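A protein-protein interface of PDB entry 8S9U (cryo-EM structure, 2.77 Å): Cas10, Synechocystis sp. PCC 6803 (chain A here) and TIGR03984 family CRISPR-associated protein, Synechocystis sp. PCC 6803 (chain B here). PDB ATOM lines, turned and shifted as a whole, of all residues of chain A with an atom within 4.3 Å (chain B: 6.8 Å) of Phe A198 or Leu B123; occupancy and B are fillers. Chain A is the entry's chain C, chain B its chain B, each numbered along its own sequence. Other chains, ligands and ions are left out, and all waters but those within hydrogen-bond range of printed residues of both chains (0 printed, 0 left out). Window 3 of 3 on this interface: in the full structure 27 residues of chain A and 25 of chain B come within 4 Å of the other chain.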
ATOM      1  N   ALA A 185     -25.585 -31.052 -24.737  1.00  0.00           N
ATOM      2  CA  ALA A 185     -25.095 -29.911 -23.976  1.00  0.00           C
ATOM      3  C   ALA A 185     -26.199 -28.900 -23.716  1.00  0.00           C
ATOM      4  O   ALA A 185     -27.120 -28.732 -24.514  1.00  0.00           O
ATOM      5  CB  ALA A 185     -23.936 -29.231 -24.697  1.00  0.00           C
ATOM      6  N   ALA A 186     -26.091 -28.217 -22.585  1.00  0.00           N
ATOM      7  CA  ALA A 186     -27.093 -27.250 -22.188  1.00  0.00           C
ATOM      8  C   ALA A 186     -26.794 -25.918 -22.846  1.00  0.00           C
ATOM      9  O   ALA A 186     -25.711 -25.693 -23.383  1.00  0.00           O
ATOM     10  CB  ALA A 186     -27.133 -27.090 -20.676  1.00  0.00           C
ATOM     11  N   ALA A 195     -23.676 -24.103 -22.741  1.00  0.00           N
ATOM     12  CA  ALA A 195     -23.169 -23.789 -21.417  1.00  0.00           C
ATOM     13  C   ALA A 195     -21.967 -24.648 -21.082  1.00  0.00           C
ATOM     14  O   ALA A 195     -21.893 -25.818 -21.454  1.00  0.00           O
ATOM     15  CB  ALA A 195     -24.250 -23.993 -20.366  1.00  0.00           C
ATOM     16  N   SER A 196     -21.026 -24.051 -20.363  1.00  0.00           N
ATOM     17  CA  SER A 196     -19.765 -24.689 -20.007  1.00  0.00           C
ATOM     18  C   SER A 196     -19.334 -24.391 -18.587  1.00  0.00           C
ATOM     19  O   SER A 196     -18.520 -25.138 -18.035  1.00  0.00           O
ATOM     20  CB  SER A 196     -18.657 -24.256 -20.963  1.00  0.00           C
ATOM     21  OG  SER A 196     -17.390 -24.607 -20.447  1.00  0.00           O
ATOM     22  N   ASP A 197     -19.834 -23.319 -17.989  1.00  0.00           N
ATOM     23  CA  ASP A 197     -19.431 -22.814 -16.692  1.00  0.00           C
ATOM     24  C   ASP A 197     -20.690 -22.297 -16.027  1.00  0.00           C
ATOM     25  O   ASP A 197     -21.756 -22.239 -16.640  1.00  0.00           O
ATOM     26  CB  ASP A 197     -18.384 -21.700 -16.783  1.00  0.00           C
ATOM     27  CG  ASP A 197     -17.150 -22.112 -17.552  1.00  0.00           C
ATOM     28  OD1 ASP A 197     -17.178 -22.063 -18.797  1.00  0.00           O
ATOM     29  OD2 ASP A 197     -16.142 -22.472 -16.912  1.00  0.00           O
ATOM     30  N   PHE A 198     -20.579 -21.965 -14.753  1.00  0.00           N
ATOM     31  CA  PHE A 198     -21.645 -21.265 -14.063  1.00  0.00           C
ATOM     32  C   PHE A 198     -21.184 -19.868 -13.678  1.00  0.00           C
ATOM     33  O   PHE A 198     -20.001 -19.629 -13.434  1.00  0.00           O
ATOM     34  CB  PHE A 198     -22.098 -22.026 -12.823  1.00  0.00           C
ATOM     35  CG  PHE A 198     -23.027 -23.156 -13.116  1.00  0.00           C
ATOM     36  CD1 PHE A 198     -24.378 -22.931 -13.252  1.00  0.00           C
ATOM     37  CD2 PHE A 198     -22.552 -24.440 -13.256  1.00  0.00           C
ATOM     38  CE1 PHE A 198     -25.236 -23.962 -13.512  1.00  0.00           C
ATOM     39  CE2 PHE A 198     -23.408 -25.470 -13.521  1.00  0.00           C
ATOM     40  CZ  PHE A 198     -24.751 -25.229 -13.649  1.00  0.00           C
ATOM     41  N   ASP A 199     -22.134 -18.944 -13.647  1.00  0.00           N
ATOM     42  CA  ASP A 199     -21.879 -17.598 -13.172  1.00  0.00           C
ATOM     43  C   ASP A 199     -23.158 -17.092 -12.535  1.00  0.00           C
ATOM     44  O   ASP A 199     -24.153 -17.812 -12.448  1.00  0.00           O
ATOM     45  CB  ASP A 199     -21.418 -16.681 -14.302  1.00  0.00           C
ATOM     46  CG  ASP A 199     -20.646 -15.486 -13.799  1.00  0.00           C
ATOM     47  OD1 ASP A 199     -19.415 -15.595 -13.632  1.00  0.00           O
ATOM     48  OD2 ASP A 199     -21.279 -14.443 -13.544  1.00  0.00           O
ATOM     49  N   LYS A 206     -27.184 -18.368  -9.510  1.00  0.00           N
ATOM     50  CA  LYS A 206     -26.258 -19.076 -10.377  1.00  0.00           C
ATOM     51  C   LYS A 206     -26.963 -19.478 -11.665  1.00  0.00           C
ATOM     52  O   LYS A 206     -28.101 -19.954 -11.651  1.00  0.00           O
ATOM     53  CB  LYS A 206     -25.684 -20.304  -9.678  1.00  0.00           C
ATOM     54  CG  LYS A 206     -24.369 -20.763 -10.281  1.00  0.00           C
ATOM     55  CD  LYS A 206     -23.910 -22.098  -9.725  1.00  0.00           C
ATOM     56  CE  LYS A 206     -23.519 -22.002  -8.270  1.00  0.00           C
ATOM     57  NZ  LYS A 206     -22.944 -23.289  -7.792  1.00  0.00           N
ATOM     58  N   ILE A 207     -26.268 -19.295 -12.784  1.00  0.00           N
ATOM     59  CA  ILE A 207     -26.836 -19.535 -14.110  1.00  0.00           C
ATOM     60  C   ILE A 207     -25.781 -20.168 -14.988  1.00  0.00           C
ATOM     61  O   ILE A 207     -24.575 -19.964 -14.798  1.00  0.00           O
ATOM     62  CB  ILE A 207     -27.340 -18.234 -14.767  1.00  0.00           C
ATOM     63  CG1 ILE A 207     -26.248 -17.170 -14.749  1.00  0.00           C
ATOM     64  CG2 ILE A 207     -28.599 -17.735 -14.092  1.00  0.00           C
ATOM     65  CD1 ILE A 207     -26.371 -16.149 -15.839  1.00  0.00           C
ATOM     66  N   PRO A 208     -26.210 -20.963 -15.968  1.00  0.00           N
ATOM     67  CA  PRO A 208     -25.252 -21.533 -16.920  1.00  0.00           C
ATOM     68  C   PRO A 208     -24.781 -20.482 -17.912  1.00  0.00           C
ATOM     69  O   PRO A 208     -25.576 -19.707 -18.445  1.00  0.00           O
ATOM     70  CB  PRO A 208     -26.056 -22.638 -17.607  1.00  0.00           C
ATOM     71  CG  PRO A 208     -27.453 -22.173 -17.524  1.00  0.00           C
ATOM     72  CD  PRO A 208     -27.583 -21.422 -16.233  1.00  0.00           C
ATOM     73  N   VAL A 209     -23.475 -20.454 -18.149  1.00  0.00           N
ATOM     74  CA  VAL A 209     -22.867 -19.502 -19.062  1.00  0.00           C
ATOM     75  C   VAL A 209     -21.813 -20.232 -19.874  1.00  0.00           C
ATOM     76  O   VAL A 209     -21.294 -21.271 -19.476  1.00  0.00           O
ATOM     77  CB  VAL A 209     -22.240 -18.275 -18.357  1.00  0.00           C
ATOM     78  CG1 VAL A 209     -23.273 -17.518 -17.563  1.00  0.00           C
ATOM     79  CG2 VAL A 209     -21.092 -18.696 -17.480  1.00  0.00           C
ATOM     80  N   LYS A 214     -18.102 -16.440 -19.646  1.00  0.00           N
ATOM     81  CA  LYS A 214     -17.389 -16.524 -18.377  1.00  0.00           C
ATOM     82  C   LYS A 214     -16.096 -15.713 -18.392  1.00  0.00           C
ATOM     83  O   LYS A 214     -15.802 -14.984 -17.441  1.00  0.00           O
ATOM     84  CB  LYS A 214     -17.107 -17.986 -18.047  1.00  0.00           C
ATOM     85  CG  LYS A 214     -16.580 -18.222 -16.655  1.00  0.00           C
ATOM     86  CD  LYS A 214     -17.674 -18.030 -15.632  1.00  0.00           C
ATOM     87  CE  LYS A 214     -17.168 -18.338 -14.239  1.00  0.00           C
ATOM     88  NZ  LYS A 214     -18.221 -18.128 -13.220  1.00  0.00           N
ATOM     89  N   GLN B 121     -15.293 -27.977 -21.038  1.00  0.00           N
ATOM     90  CA  GLN B 121     -16.419 -28.645 -20.416  1.00  0.00           C
ATOM     91  C   GLN B 121     -17.674 -28.257 -21.166  1.00  0.00           C
ATOM     92  O   GLN B 121     -17.695 -27.269 -21.898  1.00  0.00           O
ATOM     93  CB  GLN B 121     -16.591 -28.270 -18.948  1.00  0.00           C
ATOM     94  CG  GLN B 121     -15.364 -28.385 -18.109  1.00  0.00           C
ATOM     95  CD  GLN B 121     -15.690 -28.204 -16.656  1.00  0.00           C
ATOM     96  OE1 GLN B 121     -15.271 -28.990 -15.809  1.00  0.00           O
ATOM     97  NE2 GLN B 121     -16.454 -27.164 -16.353  1.00  0.00           N
ATOM     98  N   TYR B 122     -18.741 -29.005 -20.929  1.00  0.00           N
ATOM     99  CA  TYR B 122     -20.019 -28.704 -21.555  1.00  0.00           C
ATOM    100  C   TYR B 122     -21.093 -29.206 -20.611  1.00  0.00           C
ATOM    101  O   TYR B 122     -21.295 -30.413 -20.490  1.00  0.00           O
ATOM    102  CB  TYR B 122     -20.138 -29.378 -22.914  1.00  0.00           C
ATOM    103  CG  TYR B 122     -19.216 -28.808 -23.949  1.00  0.00           C
ATOM    104  CD1 TYR B 122     -19.359 -27.508 -24.398  1.00  0.00           C
ATOM    105  CD2 TYR B 122     -18.183 -29.564 -24.458  1.00  0.00           C
ATOM    106  CE1 TYR B 122     -18.500 -26.986 -25.325  1.00  0.00           C
ATOM    107  CE2 TYR B 122     -17.329 -29.052 -25.377  1.00  0.00           C
ATOM    108  CZ  TYR B 122     -17.490 -27.765 -25.812  1.00  0.00           C
ATOM    109  OH  TYR B 122     -16.623 -27.260 -26.744  1.00  0.00           O
ATOM    110  N   LEU B 123     -21.772 -28.289 -19.946  1.00  0.00           N
ATOM    111  CA  LEU B 123     -22.823 -28.681 -19.032  1.00  0.00           C
ATOM    112  C   LEU B 123     -23.951 -29.337 -19.811  1.00  0.00           C
ATOM    113  O   LEU B 123     -24.401 -28.809 -20.829  1.00  0.00           O
ATOM    114  CB  LEU B 123     -23.327 -27.458 -18.275  1.00  0.00           C
ATOM    115  CG  LEU B 123     -24.613 -27.571 -17.465  1.00  0.00           C
ATOM    116  CD1 LEU B 123     -24.361 -28.270 -16.151  1.00  0.00           C
ATOM    117  CD2 LEU B 123     -25.210 -26.205 -17.253  1.00  0.00           C
ATOM    118  N   LEU B 124     -24.403 -30.490 -19.341  1.00  0.00           N
ATOM    119  CA  LEU B 124     -25.499 -31.189 -19.980  1.00  0.00           C
ATOM    120  C   LEU B 124     -26.834 -30.672 -19.467  1.00  0.00           C
ATOM    121  O   LEU B 124     -26.914 -29.907 -18.509  1.00  0.00           O
ATOM    122  CB  LEU B 124     -25.400 -32.699 -19.775  1.00  0.00           C
ATOM    123  CG  LEU B 124     -24.052 -33.392 -19.903  1.00  0.00           C
ATOM    124  CD1 LEU B 124     -24.237 -34.879 -19.796  1.00  0.00           C
ATOM    125  CD2 LEU B 124     -23.394 -33.049 -21.206  1.00  0.00           C
ATOM    126  N   TRP B 125     -27.894 -31.108 -20.124  1.00  0.00           N
ATOM    127  CA  TRP B 125     -29.236 -30.634 -19.835  1.00  0.00           C
ATOM    128  C   TRP B 125     -29.797 -31.322 -18.604  1.00  0.00           C
ATOM    129  O   TRP B 125     -29.883 -32.552 -18.569  1.00  0.00           O
ATOM    130  CB  TRP B 125     -30.162 -30.968 -20.995  1.00  0.00           C
ATOM    131  CG  TRP B 125     -30.085 -30.199 -22.230  1.00  0.00           C
ATOM    132  CD1 TRP B 125     -29.639 -30.632 -23.429  1.00  0.00           C
ATOM    133  CD2 TRP B 125     -30.580 -28.882 -22.436  1.00  0.00           C
ATOM    134  NE1 TRP B 125     -29.773 -29.646 -24.366  1.00  0.00           N
ATOM    135  CE2 TRP B 125     -30.352 -28.558 -23.776  1.00  0.00           C
ATOM    136  CE3 TRP B 125     -31.169 -27.934 -21.608  1.00  0.00           C
ATOM    137  CZ2 TRP B 125     -30.693 -27.330 -24.306  1.00  0.00           C
ATOM    138  CZ3 TRP B 125     -31.499 -26.729 -22.133  1.00  0.00           C
ATOM    139  CH2 TRP B 125     -31.266 -26.431 -23.466  1.00  0.00           C
ATOM    140  N   GLY B 126     -30.192 -30.558 -17.604  1.00  0.00           N
ATOM    141  CA  GLY B 126     -30.917 -31.231 -16.553  1.00  0.00           C
ATOM    142  C   GLY B 126     -30.150 -31.299 -15.245  1.00  0.00           C
ATOM    143  O   GLY B 126     -28.924 -31.172 -15.190  1.00  0.00           O
ATOM    144  N   ARG B 162     -24.156 -31.541 -11.009  1.00  0.00           N
ATOM    145  CA  ARG B 162     -24.402 -31.291 -12.417  1.00  0.00           C
ATOM    146  C   ARG B 162     -23.397 -32.113 -13.193  1.00  0.00           C
ATOM    147  O   ARG B 162     -22.237 -32.225 -12.793  1.00  0.00           O
ATOM    148  CB  ARG B 162     -24.270 -29.819 -12.806  1.00  0.00           C
ATOM    149  CG  ARG B 162     -25.173 -28.895 -12.058  1.00  0.00           C
ATOM    150  CD  ARG B 162     -26.607 -29.150 -12.404  1.00  0.00           C
ATOM    151  NE  ARG B 162     -27.490 -28.370 -11.548  1.00  0.00           N
ATOM    152  CZ  ARG B 162     -28.213 -28.883 -10.559  1.00  0.00           C
ATOM    153  NH1 ARG B 162     -28.122 -30.172 -10.267  1.00  0.00           N
ATOM    154  NH2 ARG B 162     -28.995 -28.097  -9.832  1.00  0.00           N
ATOM    155  N   VAL B 163     -23.836 -32.670 -14.305  1.00  0.00           N
ATOM    156  CA  VAL B 163     -23.010 -33.553 -15.106  1.00  0.00           C
ATOM    157  C   VAL B 163     -22.447 -32.746 -16.254  1.00  0.00           C
ATOM    158  O   VAL B 163     -23.180 -32.014 -16.928  1.00  0.00           O
ATOM    159  CB  VAL B 163     -23.810 -34.760 -15.614  1.00  0.00           C
ATOM    160  CG1 VAL B 163     -22.919 -35.683 -16.390  1.00  0.00           C
ATOM    161  CG2 VAL B 163     -24.435 -35.483 -14.457  1.00  0.00           C
ATOM    162  N   PHE B 164     -21.144 -32.855 -16.459  1.00  0.00           N
ATOM    163  CA  PHE B 164     -20.443 -32.118 -17.485  1.00  0.00           C
ATOM    164  C   PHE B 164     -19.843 -33.123 -18.450  1.00  0.00           C
ATOM    165  O   PHE B 164     -19.645 -34.289 -18.113  1.00  0.00           O
ATOM    166  CB  PHE B 164     -19.322 -31.276 -16.875  1.00  0.00           C
ATOM    167  CG  PHE B 164     -19.780 -29.985 -16.282  1.00  0.00           C
ATOM    168  CD1 PHE B 164     -20.305 -29.951 -15.013  1.00  0.00           C
ATOM    169  CD2 PHE B 164     -19.639 -28.801 -16.966  1.00  0.00           C
ATOM    170  CE1 PHE B 164     -20.714 -28.778 -14.460  1.00  0.00           C
ATOM    171  CE2 PHE B 164     -20.051 -27.624 -16.412  1.00  0.00           C
ATOM    172  CZ  PHE B 164     -20.586 -27.613 -15.158  1.00  0.00           C
ATOM    173  N   LEU B 165     -19.550 -32.665 -19.656  1.00  0.00           N
ATOM    174  CA  LEU B 165     -18.841 -33.470 -20.633  1.00  0.00           C
ATOM    175  C   LEU B 165     -17.533 -32.752 -20.915  1.00  0.00           C
ATOM    176  O   LEU B 165     -17.535 -31.550 -21.186  1.00  0.00           O
ATOM    177  CB  LEU B 165     -19.691 -33.658 -21.888  1.00  0.00           C
ATOM    178  CG  LEU B 165     -19.114 -34.131 -23.213  1.00  0.00           C
ATOM    179  CD1 LEU B 165     -18.380 -35.428 -23.051  1.00  0.00           C
ATOM    180  CD2 LEU B 165     -20.262 -34.330 -24.145  1.00  0.00           C
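The backbone carbonyl oxygen of Gln B121 lies within hydrogen-bond range of the side-chain hydroxyl of Ser A196, at 3.0 Å.
O of Leu B123 lies within hydrogen-bond range of N of Ala A186, 2.5 Å away.
The backbone NH (N) of Leu B123 lies within hydrogen-bond range of the backbone carbonyl oxygen (O) of Ala A195 (2.9 Å).
The indole nitrogen of Trp B125 sits at hydrogen-bond distance from the backbone carbonyl oxygen of Ala A185 (2.8 Å).
The backbone carbonyl oxygen of Leu B165 is in hydrogen-bond range of the backbone NH of Tyr B122.
The backbone carbonyl oxygen (O) of Val B163 sits at hydrogen-bond distance from the backbone NH (N) of Leu B124, 3.1 Å away.
The backbone NH (N) of Ala A195 sits at hydrogen-bond distance from the backbone carbonyl oxygen (O) of Ala A186.
OG of Ser A196 is in hydrogen-bond range of OD1 of Asp A197 (3.0 Å).
The backbone NH (N) of Ser A196 is in hydrogen-bond range of the backbone carbonyl oxygen (O) of Val A209 (2.9 Å).
Ala A185 touches Leu B123.
CB of Ala A186 touches O of Leu B124, at 3.6 Å.
CE2 of Trp B125 touches CA of Ala A186, 3.9 Å away.
CA of Tyr B122 touches O of Ala A195, at 3.4 Å.
O of Ser A196 touches CE2 of Phe B164, 3.3 Å away.
CD2 of Leu B123 touches CZ of Phe A198, 3.8 Å away.
Phe B164 touches Phe A198 (CZ to CE2, 3.9 Å).
Pro A208 touches Leu B123 (CB to CD2, 3.7 Å).
Asp A197 touches none of the printed residues of chain B.
Of the printed residues of chain A, Gln B121 touches Ser A196 (3.0 Å).
Leu B123 touches just these residues of chain A: Ala A185 (3.4 Å), Ala A186 (2.5 Å), Ala A195 (2.9 Å), Phe A198 (3.8 Å) and Pro A208 (3.7 Å).
Of the printed residues of chain A, Trp B125 touches Ala A185 (2.8 Å) and Ala A186 (3.9 Å).
Gly B126 touches none of the printed residues of chain A.
The nearest printed residue of chain B that does not touch Phe A198 is Arg B162 (4.02 Å).
The nearest residue of chain A that does not touch Leu B123 is Ser A196 (4.1 Å).
Of the 12 printed residues of chain A, 6 touch a printed residue of chain B.
Hydrophobic or aromatic side chains of chain A that line the printed part of chain B: Ala A185, Ala A186, Ala A195, Phe A198 and Pro A208.
Of the 10 printed residues of chain B, 6 touch a printed residue of chain A.
Among the printed residues, no Asp or Glu carboxylate lies within 4 Å of a Lys or Arg side-chain nitrogen of the other chain.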
